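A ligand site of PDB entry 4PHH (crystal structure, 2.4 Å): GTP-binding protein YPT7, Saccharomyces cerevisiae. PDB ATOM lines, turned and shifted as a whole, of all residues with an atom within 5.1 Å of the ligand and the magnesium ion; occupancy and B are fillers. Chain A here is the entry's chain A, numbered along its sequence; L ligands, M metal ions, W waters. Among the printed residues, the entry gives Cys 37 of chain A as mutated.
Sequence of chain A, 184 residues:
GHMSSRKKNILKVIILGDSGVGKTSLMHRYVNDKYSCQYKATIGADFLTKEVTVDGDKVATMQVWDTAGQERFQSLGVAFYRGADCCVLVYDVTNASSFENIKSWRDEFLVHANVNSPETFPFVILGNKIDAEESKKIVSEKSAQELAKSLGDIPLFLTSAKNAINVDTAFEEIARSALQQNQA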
ATOM      1  N   GLY A  17      27.332  13.849  18.871  1.00  0.00           N
ATOM      2  CA  GLY A  17      26.783  15.197  18.995  1.00  0.00           C
ATOM      3  C   GLY A  17      27.288  15.798  20.287  1.00  0.00           C
ATOM      4  O   GLY A  17      27.837  15.081  21.116  1.00  0.00           O
ATOM      5  N   ASP A  18      27.107  17.107  20.440  1.00  0.00           N
ATOM      6  CA  ASP A  18      27.599  17.818  21.628  1.00  0.00           C
ATOM      7  C   ASP A  18      27.063  17.325  22.965  1.00  0.00           C
ATOM      8  O   ASP A  18      26.028  16.663  23.050  1.00  0.00           O
ATOM      9  CB  ASP A  18      27.362  19.339  21.522  1.00  0.00           C
ATOM     10  CG  ASP A  18      28.206  19.972  20.403  1.00  0.00           C
ATOM     11  OD1 ASP A  18      29.062  19.244  19.760  1.00  0.00           O
ATOM     12  OD2 ASP A  18      27.992  21.192  20.162  1.00  0.00           O
ATOM     13  N   SER A  19      27.794  17.649  24.024  1.00  0.00           N
ATOM     14  CA  SER A  19      27.330  17.405  25.394  1.00  0.00           C
ATOM     15  C   SER A  19      26.002  18.104  25.646  1.00  0.00           C
ATOM     16  O   SER A  19      25.817  19.267  25.345  1.00  0.00           O
ATOM     17  CB  SER A  19      28.378  17.870  26.413  1.00  0.00           C
ATOM     18  OG  SER A  19      28.031  17.473  27.750  1.00  0.00           O
ATOM     19  N   GLY A  20      25.050  17.363  26.153  1.00  0.00           N
ATOM     20  CA  GLY A  20      23.811  17.931  26.603  1.00  0.00           C
ATOM     21  C   GLY A  20      22.683  17.768  25.643  1.00  0.00           C
ATOM     22  O   GLY A  20      21.543  18.039  26.029  1.00  0.00           O
ATOM     23  N   VAL A  21      22.975  17.349  24.403  1.00  0.00           N
ATOM     24  CA  VAL A  21      21.941  17.331  23.335  1.00  0.00           C
ATOM     25  C   VAL A  21      20.905  16.232  23.539  1.00  0.00           C
ATOM     26  O   VAL A  21      19.799  16.294  22.951  1.00  0.00           O
ATOM     27  CB  VAL A  21      22.524  17.195  21.867  1.00  0.00           C
ATOM     28  CG1 VAL A  21      23.424  18.358  21.517  1.00  0.00           C
ATOM     29  CG2 VAL A  21      23.236  15.837  21.617  1.00  0.00           C
ATOM     30  N   GLY A  22      21.256  15.214  24.325  1.00  0.00           N
ATOM     31  CA  GLY A  22      20.364  14.135  24.645  1.00  0.00           C
ATOM     32  C   GLY A  22      20.642  12.754  24.042  1.00  0.00           C
ATOM     33  O   GLY A  22      19.729  11.963  23.944  1.00  0.00           O
ATOM     34  N   LYS A  23      21.895  12.436  23.702  1.00  0.00           N
ATOM     35  CA  LYS A  23      22.274  11.129  23.105  1.00  0.00           C
ATOM     36  C   LYS A  23      21.974   9.908  23.969  1.00  0.00           C
ATOM     37  O   LYS A  23      21.456   8.911  23.470  1.00  0.00           O
ATOM     38  CB  LYS A  23      23.782  11.103  22.772  1.00  0.00           C
ATOM     39  CG  LYS A  23      24.220  12.186  21.784  1.00  0.00           C
ATOM     40  CD  LYS A  23      25.729  12.171  21.515  1.00  0.00           C
ATOM     41  CE  LYS A  23      26.594  12.577  22.701  1.00  0.00           C
ATOM     42  NZ  LYS A  23      26.242  13.926  23.264  1.00  0.00           N
ATOM     43  N   THR A  24      22.382   9.989  25.240  1.00  0.00           N
ATOM     44  CA  THR A  24      22.207   8.922  26.201  1.00  0.00           C
ATOM     45  C   THR A  24      20.685   8.777  26.406  1.00  0.00           C
ATOM     46  O   THR A  24      20.153   7.654  26.313  1.00  0.00           O
ATOM     47  CB  THR A  24      22.981   9.209  27.531  1.00  0.00           C
ATOM     48  OG1 THR A  24      24.371   9.531  27.269  1.00  0.00           O
ATOM     49  CG2 THR A  24      22.966   8.005  28.477  1.00  0.00           C
ATOM     50  N   SER A  25      19.981   9.882  26.597  1.00  0.00           N
ATOM     51  CA  SER A  25      18.525   9.802  26.733  1.00  0.00           C
ATOM     52  C   SER A  25      17.875   9.156  25.545  1.00  0.00           C
ATOM     53  O   SER A  25      16.920   8.412  25.692  1.00  0.00           O
ATOM     54  CB  SER A  25      17.882  11.167  26.872  1.00  0.00           C
ATOM     55  OG  SER A  25      18.436  11.890  27.920  1.00  0.00           O
ATOM     56  N   LEU A  26      18.319   9.467  24.344  1.00  0.00           N
ATOM     57  CA  LEU A  26      17.666   8.880  23.152  1.00  0.00           C
ATOM     58  C   LEU A  26      17.912   7.352  23.101  1.00  0.00           C
ATOM     59  O   LEU A  26      17.050   6.590  22.676  1.00  0.00           O
ATOM     60  CB  LEU A  26      18.197   9.525  21.893  1.00  0.00           C
ATOM     61  CG  LEU A  26      17.738  10.957  21.637  1.00  0.00           C
ATOM     62  CD1 LEU A  26      18.714  11.684  20.686  1.00  0.00           C
ATOM     63  CD2 LEU A  26      16.302  11.007  21.100  1.00  0.00           C
ATOM     64  N   TYR A  35      13.013   7.108  30.518  1.00  0.00           N
ATOM     65  CA  TYR A  35      13.657   8.419  30.531  1.00  0.00           C
ATOM     66  C   TYR A  35      13.818   8.966  31.972  1.00  0.00           C
ATOM     67  O   TYR A  35      12.979   8.737  32.862  1.00  0.00           O
ATOM     68  CB  TYR A  35      12.891   9.436  29.653  1.00  0.00           C
ATOM     69  CG  TYR A  35      13.323  10.877  29.878  1.00  0.00           C
ATOM     70  CD1 TYR A  35      14.338  11.460  29.122  1.00  0.00           C
ATOM     71  CD2 TYR A  35      12.720  11.649  30.870  1.00  0.00           C
ATOM     72  CE1 TYR A  35      14.733  12.775  29.342  1.00  0.00           C
ATOM     73  CE2 TYR A  35      13.107  12.966  31.105  1.00  0.00           C
ATOM     74  CZ  TYR A  35      14.114  13.521  30.337  1.00  0.00           C
ATOM     75  OH  TYR A  35      14.482  14.834  30.577  1.00  0.00           O
ATOM     76  N   SER A  36      14.889   9.712  32.185  1.00  0.00           N
ATOM     77  CA  SER A  36      15.218  10.292  33.463  1.00  0.00           C
ATOM     78  C   SER A  36      15.688  11.762  33.296  1.00  0.00           C
ATOM     79  O   SER A  36      16.507  12.072  32.441  1.00  0.00           O
ATOM     80  CB  SER A  36      16.305   9.437  34.090  1.00  0.00           C
ATOM     81  OG  SER A  36      16.579   9.859  35.399  1.00  0.00           O
ATOM     82  N   CYS A  37      15.178  12.657  34.112  1.00  0.00           N
ATOM     83  CA  CYS A  37      15.523  14.091  34.012  1.00  0.00           C
ATOM     84  C   CYS A  37      16.982  14.370  34.381  1.00  0.00           C
ATOM     85  O   CYS A  37      17.530  15.427  34.042  1.00  0.00           O
ATOM     86  CB  CYS A  37      14.628  14.917  34.959  1.00  0.00           C
ATOM     87  SG  CYS A  37      12.948  15.244  34.370  1.00  0.00           S
ATOM     88  N   GLN A  38      17.602  13.439  35.092  1.00  0.00           N
ATOM     89  CA  GLN A  38      18.861  13.702  35.736  1.00  0.00           C
ATOM     90  C   GLN A  38      20.027  13.532  34.777  1.00  0.00           C
ATOM     91  O   GLN A  38      20.334  12.416  34.321  1.00  0.00           O
ATOM     92  CB  GLN A  38      19.039  12.818  36.968  1.00  0.00           C
ATOM     93  CG  GLN A  38      20.085  13.311  37.956  1.00  0.00           C
ATOM     94  CD  GLN A  38      19.923  14.782  38.300  1.00  0.00           C
ATOM     95  OE1 GLN A  38      18.832  15.241  38.660  1.00  0.00           O
ATOM     96  NE2 GLN A  38      21.014  15.538  38.175  1.00  0.00           N
ATOM     97  N   TYR A  39      20.673  14.666  34.480  1.00  0.00           N
ATOM     98  CA  TYR A  39      21.899  14.676  33.685  1.00  0.00           C
ATOM     99  C   TYR A  39      23.013  13.865  34.383  1.00  0.00           C
ATOM    100  O   TYR A  39      23.429  14.184  35.527  1.00  0.00           O
ATOM    101  CB  TYR A  39      22.365  16.116  33.423  1.00  0.00           C
ATOM    102  CG  TYR A  39      23.646  16.229  32.593  1.00  0.00           C
ATOM    103  CD1 TYR A  39      24.771  16.908  33.092  1.00  0.00           C
ATOM    104  CD2 TYR A  39      23.746  15.650  31.321  1.00  0.00           C
ATOM    105  CE1 TYR A  39      25.940  17.005  32.358  1.00  0.00           C
ATOM    106  CE2 TYR A  39      24.910  15.756  30.570  1.00  0.00           C
ATOM    107  CZ  TYR A  39      26.000  16.427  31.099  1.00  0.00           C
ATOM    108  OH  TYR A  39      27.166  16.538  30.361  1.00  0.00           O
ATOM    109  N   LYS A  40      23.436  12.798  33.684  1.00  0.00           N
ATOM    110  CA  LYS A  40      24.591  11.973  34.072  1.00  0.00           C
ATOM    111  C   LYS A  40      25.583  11.908  32.883  1.00  0.00           C
ATOM    112  O   LYS A  40      25.382  11.118  31.959  1.00  0.00           O
ATOM    113  CB  LYS A  40      24.131  10.556  34.483  1.00  0.00           C
ATOM    114  N   ALA A  41      26.657  12.728  32.934  1.00  0.00           N
ATOM    115  CA  ALA A  41      27.623  12.848  31.799  1.00  0.00           C
ATOM    116  C   ALA A  41      28.195  11.506  31.345  1.00  0.00           C
ATOM    117  O   ALA A  41      28.724  10.742  32.133  1.00  0.00           O
ATOM    118  CB  ALA A  41      28.776  13.783  32.139  1.00  0.00           C
ATOM    119  N   THR A  42      28.104  11.228  30.051  1.00  0.00           N
ATOM    120  CA  THR A  42      28.713  10.043  29.478  1.00  0.00           C
ATOM    121  C   THR A  42      30.252  10.167  29.338  1.00  0.00           C
ATOM    122  O   THR A  42      30.800  11.192  28.867  1.00  0.00           O
ATOM    123  CB  THR A  42      28.173   9.758  28.077  1.00  0.00           C
ATOM    124  OG1 THR A  42      26.731   9.821  28.117  1.00  0.00           O
ATOM    125  CG2 THR A  42      28.677   8.391  27.573  1.00  0.00           C
ATOM    126  N   ASP A  66      26.824   4.757  22.553  1.00  0.00           N
ATOM    127  CA  ASP A  66      26.740   6.105  23.102  1.00  0.00           C
ATOM    128  C   ASP A  66      28.163   6.590  23.353  1.00  0.00           C
ATOM    129  O   ASP A  66      29.034   5.813  23.772  1.00  0.00           O
ATOM    130  CB  ASP A  66      25.902   6.060  24.374  1.00  0.00           C
ATOM    131  CG  ASP A  66      25.474   7.452  24.866  1.00  0.00           C
ATOM    132  OD1 ASP A  66      25.615   8.433  24.105  1.00  0.00           O
ATOM    133  OD2 ASP A  66      24.994   7.531  26.030  1.00  0.00           O
ATOM    134  N   THR A  67      28.392   7.869  23.097  1.00  0.00           N
ATOM    135  CA  THR A  67      29.725   8.448  23.155  1.00  0.00           C
ATOM    136  C   THR A  67      29.676   9.707  23.985  1.00  0.00           C
ATOM    137  O   THR A  67      28.634  10.276  24.188  1.00  0.00           O
ATOM    138  CB  THR A  67      30.269   8.791  21.718  1.00  0.00           C
ATOM    139  OG1 THR A  67      29.439   9.780  21.055  1.00  0.00           O
ATOM    140  CG2 THR A  67      30.355   7.535  20.867  1.00  0.00           C
ATOM    141  N   ALA A  68      30.816  10.167  24.451  1.00  0.00           N
ATOM    142  CA  ALA A  68      30.848  11.373  25.264  1.00  0.00           C
ATOM    143  C   ALA A  68      30.815  12.590  24.351  1.00  0.00           C
ATOM    144  O   ALA A  68      31.467  12.609  23.310  1.00  0.00           O
ATOM    145  CB  ALA A  68      32.096  11.391  26.114  1.00  0.00           C
ATOM    146  N   GLY A  69      30.086  13.612  24.740  1.00  0.00           N
ATOM    147  CA  GLY A  69      30.136  14.880  24.023  1.00  0.00           C
ATOM    148  C   GLY A  69      31.252  15.809  24.476  1.00  0.00           C
ATOM    149  O   GLY A  69      31.780  16.594  23.682  1.00  0.00           O
ATOM    150  N   GLN A  70      31.590  15.730  25.758  1.00  0.00           N
ATOM    151  CA  GLN A  70      32.687  16.524  26.335  1.00  0.00           C
ATOM    152  C   GLN A  70      34.054  15.990  25.885  1.00  0.00           C
ATOM    153  O   GLN A  70      34.356  14.812  26.085  1.00  0.00           O
ATOM    154  CB  GLN A  70      32.630  16.446  27.869  1.00  0.00           C
ATOM    155  CG  GLN A  70      31.448  17.143  28.516  1.00  0.00           C
ATOM    156  CD  GLN A  70      31.517  17.095  30.037  1.00  0.00           C
ATOM    157  OE1 GLN A  70      30.537  16.836  30.724  1.00  0.00           O
ATOM    158  NE2 GLN A  70      32.683  17.334  30.559  1.00  0.00           N
ATOM    159  N   ASN A 128      16.856  17.123  18.679  1.00  0.00           N
ATOM    160  CA  ASN A 128      16.195  16.637  19.872  1.00  0.00           C
ATOM    161  C   ASN A 128      15.714  17.754  20.789  1.00  0.00           C
ATOM    162  O   ASN A 128      16.140  18.900  20.648  1.00  0.00           O
ATOM    163  CB  ASN A 128      17.151  15.699  20.590  1.00  0.00           C
ATOM    164  CG  ASN A 128      16.494  14.897  21.695  1.00  0.00           C
ATOM    165  OD1 ASN A 128      17.048  14.798  22.795  1.00  0.00           O
ATOM    166  ND2 ASN A 128      15.317  14.292  21.412  1.00  0.00           N
ATOM    167  N   LYS A 129      14.809  17.407  21.698  1.00  0.00           N
ATOM    168  CA  LYS A 129      14.251  18.300  22.725  1.00  0.00           C
ATOM    169  C   LYS A 129      13.108  19.169  22.192  1.00  0.00           C
ATOM    170  O   LYS A 129      12.910  20.292  22.675  1.00  0.00           O
ATOM    171  CB  LYS A 129      15.332  19.164  23.446  1.00  0.00           C
ATOM    172  CG  LYS A 129      16.515  18.415  24.037  1.00  0.00           C
ATOM    173  CD  LYS A 129      17.181  19.209  25.143  1.00  0.00           C
ATOM    174  CE  LYS A 129      18.434  18.527  25.641  1.00  0.00           C
ATOM    175  NZ  LYS A 129      19.164  19.359  26.641  1.00  0.00           N
ATOM    176  N   ASP A 131       9.966  18.861  22.705  1.00  0.00           N
ATOM    177  CA  ASP A 131       9.005  19.059  23.776  1.00  0.00           C
ATOM    178  C   ASP A 131       9.217  20.342  24.583  1.00  0.00           C
ATOM    179  O   ASP A 131       8.367  20.683  25.425  1.00  0.00           O
ATOM    180  CB  ASP A 131       9.145  17.919  24.777  1.00  0.00           C
ATOM    181  CG  ASP A 131      10.504  17.919  25.443  1.00  0.00           C
ATOM    182  OD1 ASP A 131      11.476  17.584  24.741  1.00  0.00           O
ATOM    183  OD2 ASP A 131      10.620  18.291  26.649  1.00  0.00           O
ATOM    184  N   ALA A 132      10.360  20.996  24.402  1.00  0.00           N
ATOM    185  CA  ALA A 132      10.688  22.198  25.191  1.00  0.00           C
ATOM    186  C   ALA A 132       9.839  23.387  24.726  1.00  0.00           C
ATOM    187  O   ALA A 132       9.305  23.372  23.609  1.00  0.00           O
ATOM    188  CB  ALA A 132      12.175  22.507  25.078  1.00  0.00           C
ATOM    189  N   THR A 159      12.864  14.983  17.357  1.00  0.00           N
ATOM    190  CA  THR A 159      12.549  13.983  18.360  1.00  0.00           C
ATOM    191  C   THR A 159      12.465  14.565  19.757  1.00  0.00           C
ATOM    192  O   THR A 159      12.920  15.681  20.021  1.00  0.00           O
ATOM    193  CB  THR A 159      13.603  12.868  18.334  1.00  0.00           C
ATOM    194  OG1 THR A 159      14.896  13.422  18.625  1.00  0.00           O
ATOM    195  CG2 THR A 159      13.626  12.189  17.001  1.00  0.00           C
ATOM    196  N   SER A 160      11.816  13.817  20.653  1.00  0.00           N
ATOM    197  CA  SER A 160      11.872  14.084  22.069  1.00  0.00           C
ATOM    198  C   SER A 160      12.103  12.781  22.750  1.00  0.00           C
ATOM    199  O   SER A 160      11.232  11.940  22.753  1.00  0.00           O
ATOM    200  CB  SER A 160      10.590  14.720  22.577  1.00  0.00           C
ATOM    201  OG  SER A 160      10.524  14.763  23.989  1.00  0.00           O
ATOM    202  N   ALA A 161      13.288  12.582  23.291  1.00  0.00           N
ATOM    203  CA  ALA A 161      13.504  11.424  24.189  1.00  0.00           C
ATOM    204  C   ALA A 161      12.587  11.534  25.434  1.00  0.00           C
ATOM    205  O   ALA A 161      12.203  10.520  25.999  1.00  0.00           O
ATOM    206  CB  ALA A 161      14.968  11.337  24.628  1.00  0.00           C
ATOM    207  N   LYS A 162      12.285  12.736  25.897  1.00  0.00           N
ATOM    208  CA  LYS A 162      11.554  12.877  27.159  1.00  0.00           C
ATOM    209  C   LYS A 162      10.122  12.381  27.056  1.00  0.00           C
ATOM    210  O   LYS A 162       9.687  11.502  27.808  1.00  0.00           O
ATOM    211  CB  LYS A 162      11.520  14.329  27.604  1.00  0.00           C
ATOM    212  CG  LYS A 162      10.642  14.566  28.809  1.00  0.00           C
ATOM    213  CD  LYS A 162      10.755  16.019  29.256  1.00  0.00           C
ATOM    214  CE  LYS A 162       9.489  16.479  29.972  1.00  0.00           C
ATOM    215  NZ  LYS A 162       9.770  17.846  30.440  1.00  0.00           N
HETATM  216  O1  LIG L   1      11.609  19.326  32.532  1.00  0.00           O
HETATM  217  C1  LIG L   1      12.745  18.920  32.788  1.00  0.00           C
HETATM  218  C2  LIG L   1      13.020  18.091  34.040  1.00  0.00           C
HETATM  219  C3  LIG L   1      12.402  16.681  33.854  1.00  0.00           C
HETATM  220  N1  LIG L   1      13.832  19.238  32.073  1.00  0.00           N
HETATM  221  C4  LIG L   1      13.762  20.082  30.869  1.00  0.00           C
HETATM  222  C5  LIG L   1      13.083  19.300  29.762  1.00  0.00           C
HETATM  223  C6  LIG L   1      13.917  19.498  28.521  1.00  0.00           C
HETATM  224  N2  LIG L   1      13.379  18.519  27.597  1.00  0.00           N
HETATM  225  C7  LIG L   1      14.101  17.503  27.131  1.00  0.00           C
HETATM  226  N3  LIG L   1      15.273  17.195  27.703  1.00  0.00           N
HETATM  227  N4  LIG L   1      13.672  16.751  26.054  1.00  0.00           N
HETATM  228  C8  LIG L   1      14.468  15.690  25.601  1.00  0.00           C
HETATM  229  O2  LIG L   1      14.065  15.022  24.627  1.00  0.00           O
HETATM  230  C9  LIG L   1      15.651  15.451  26.238  1.00  0.00           C
HETATM  231  C10 LIG L   1      16.042  16.206  27.282  1.00  0.00           C
HETATM  232  N5  LIG L   1      16.611  14.519  26.041  1.00  0.00           N
HETATM  233  C11 LIG L   1      17.572  14.738  26.954  1.00  0.00           C
HETATM  234  N6  LIG L   1      17.220  15.793  27.730  1.00  0.00           N
HETATM  235  C12 LIG L   1      17.987  16.327  28.871  1.00  0.00           C
HETATM  236  O3  LIG L   1      19.230  17.002  28.496  1.00  0.00           O
HETATM  237  C13 LIG L   1      18.364  15.208  29.831  1.00  0.00           C
HETATM  238  O4  LIG L   1      17.308  14.986  30.885  1.00  0.00           O
HETATM  239  C14 LIG L   1      19.625  15.746  30.449  1.00  0.00           C
HETATM  240  O5  LIG L   1      19.278  16.735  31.481  1.00  0.00           O
HETATM  241  C15 LIG L   1      20.323  16.505  29.346  1.00  0.00           C
HETATM  242  C16 LIG L   1      21.313  15.643  28.572  1.00  0.00           C
HETATM  243  O6  LIG L   1      20.814  14.351  28.419  1.00  0.00           O
HETATM  244  P1  LIG L   1      21.874  13.299  28.038  1.00  0.00           P
HETATM  245  O7  LIG L   1      21.056  12.216  27.369  1.00  0.00           O
HETATM  246  O8  LIG L   1      22.655  13.020  29.303  1.00  0.00           O
HETATM  247  O9  LIG L   1      22.783  14.114  26.909  1.00  0.00           O
HETATM  248  P2  LIG L   1      24.162  13.566  26.251  1.00  0.00           P
HETATM  249  O10 LIG L   1      24.154  14.077  24.873  1.00  0.00           O
HETATM  250  O11 LIG L   1      24.177  12.083  26.376  1.00  0.00           O
HETATM  251  N7  LIG L   1      25.332  14.332  27.151  1.00  0.00           N
HETATM  252  P3  LIG L   1      27.006  13.865  27.080  1.00  0.00           P
HETATM  253  O12 LIG L   1      26.844  12.509  27.579  1.00  0.00           O
HETATM  254  O13 LIG L   1      27.308  14.055  25.677  1.00  0.00           O
HETATM  255  O14 LIG L   1      27.528  14.868  27.999  1.00  0.00           O
HETATM  256 MG    MG M   1      25.505  11.018  27.356  1.00  0.00          MG
HETATM  257  O   HOH W   1      24.607  11.242  29.292  1.00  0.00           O
HETATM  258  O   HOH W   2      30.031  13.664  28.091  1.00  0.00           O
HETATM  259  O   HOH W   3      26.300  10.658  25.640  1.00  0.00           O
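The backbone NH of Gly 20 lies close to a nitrogen (N7) of the ligand (3.2 Å).
Residues that only touch the ligand: Ser 160 (3.5 Å), Val 21 (3.5 Å) and Asp 18 (3.7 Å).
Of the 31 residues printed, 20 come within 4 Å of the ligand.
The magnesium ion is bound by the side-chain hydroxyl (OG1) of Thr 24, the side-chain hydroxyl (OG1) of Thr 42, water W3, an oxygen (O11) of the ligand, an oxygen (O12) of the ligand and water W1.
The magnesium ion has six donor atoms within binding distance.
O of Cys 37 is in hydrogen-bond range of O4 of the ligand (3.2 Å).
The side-chain sulfur (SG) of Cys 37 is covalently linked to a carbon (C3) of the ligand (1.6 Å).
O7 of the ligand is in hydrogen-bond range of N of Thr 24, 3.4 Å away.
An oxygen (O12) of the ligand sits close to the backbone NH of Thr 42 (3.1 Å).
The backbone NH (N) of Lys 23 sits at hydrogen-bond distance from an oxygen (O10) of the ligand, at 3.0 Å.
The side-chain amino group of Lys 23 is in salt-bridge range of an oxygen (O10) of the ligand (2.6 Å).
O14 of the ligand sits at hydrogen-bond distance from OG of Ser 19, 2.7 Å away.
N of Ser 25 is in hydrogen-bond range of O7 of the ligand.
OG of Ser 25 lies within hydrogen-bond range of O7 of the ligand.
A nitrogen (N4) of the ligand lies within hydrogen-bond range of the side-chain carboxylate (OD1) of Asp 131 (2.7 Å).
The side-chain hydroxyl (OH) of Tyr 35 sits at hydrogen-bond distance from an oxygen (O4) of the ligand.
N of Ala 161 is in hydrogen-bond range of O2 of the ligand (2.9 Å).
An oxygen (O14) of the ligand sits at hydrogen-bond distance from the side-chain hydroxyl (OH) of Tyr 39 (2.9 Å).
An oxygen (O13) of the ligand sits at hydrogen-bond distance from the backbone NH (N) of Gly 69, 3.0 Å away.
The side-chain amino group (NZ) of Lys 129 sits at hydrogen-bond distance from an oxygen (O3) of the ligand (3.0 Å).
An oxygen (O2) of the ligand is in hydrogen-bond range of the backbone NH (N) of Lys 162 (3.2 Å).
The side-chain amino group of Lys 162 sits at hydrogen-bond distance from an oxygen (O1) of the ligand (3.2 Å).
The backbone NH (N) of Gly 22 lies within hydrogen-bond range of an oxygen (O10) of the ligand.
OD1 of Asn 128 sits close to N5 of the ligand, 3.3 Å away.
The backbone carbonyl oxygen (O) of Ser 36 lies within hydrogen-bond range of an oxygen (O4) of the ligand (3.4 Å).
Water W3 lies within hydrogen-bond range of O of Thr 67 (2.8 Å) and OD1 of Asp 66 (2.8 Å).
Water W1 lies within hydrogen-bond range of an oxygen (O8) of the ligand (2.6 Å) and the backbone carbonyl oxygen (O) of Lys 40 (2.8 Å).
Water W2 lies within hydrogen-bond range of O of Thr 42 (2.7 Å), O14 of the ligand (2.8 Å), N of Gly 69 (3.4 Å) and N of Gln 70 (3.5 Å).
The side-chain hydroxyl (OG1) of Thr 24 sits close to the side-chain carboxylate (OD2) of Asp 66 (2.4 Å).
NZ of Lys 23 is in hydrogen-bond range of O of Asp 18 (2.8 Å).
The backbone carbonyl oxygen (O) of Gly 17 lies within hydrogen-bond range of the side-chain amino group (NZ) of Lys 23, at 2.9 Å.
The side-chain amide nitrogen of Asn 128 sits close to the backbone NH of Ala 161 (3.3 Å).
The side-chain hydroxyl (OH) of Tyr 39 sits at hydrogen-bond distance from the side-chain amide oxygen (OE1) of Gln 70 (3.4 Å).
NZ of Lys 129 lies within hydrogen-bond range of O of Gly 20, at 2.8 Å.
OG of Ser 160 lies close to N of Lys 162 (3.3 Å).
The backbone carbonyl oxygen (O) of Val 21 lies close to the side-chain amide oxygen (OD1) of Asn 128 (3.1 Å).
OD2 of Asp 66 touches the magnesium ion, at 3.8 Å.
Three residues have an atom within 4 Å of the magnesium ion: Thr 24, Thr 42 and Asp 66.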
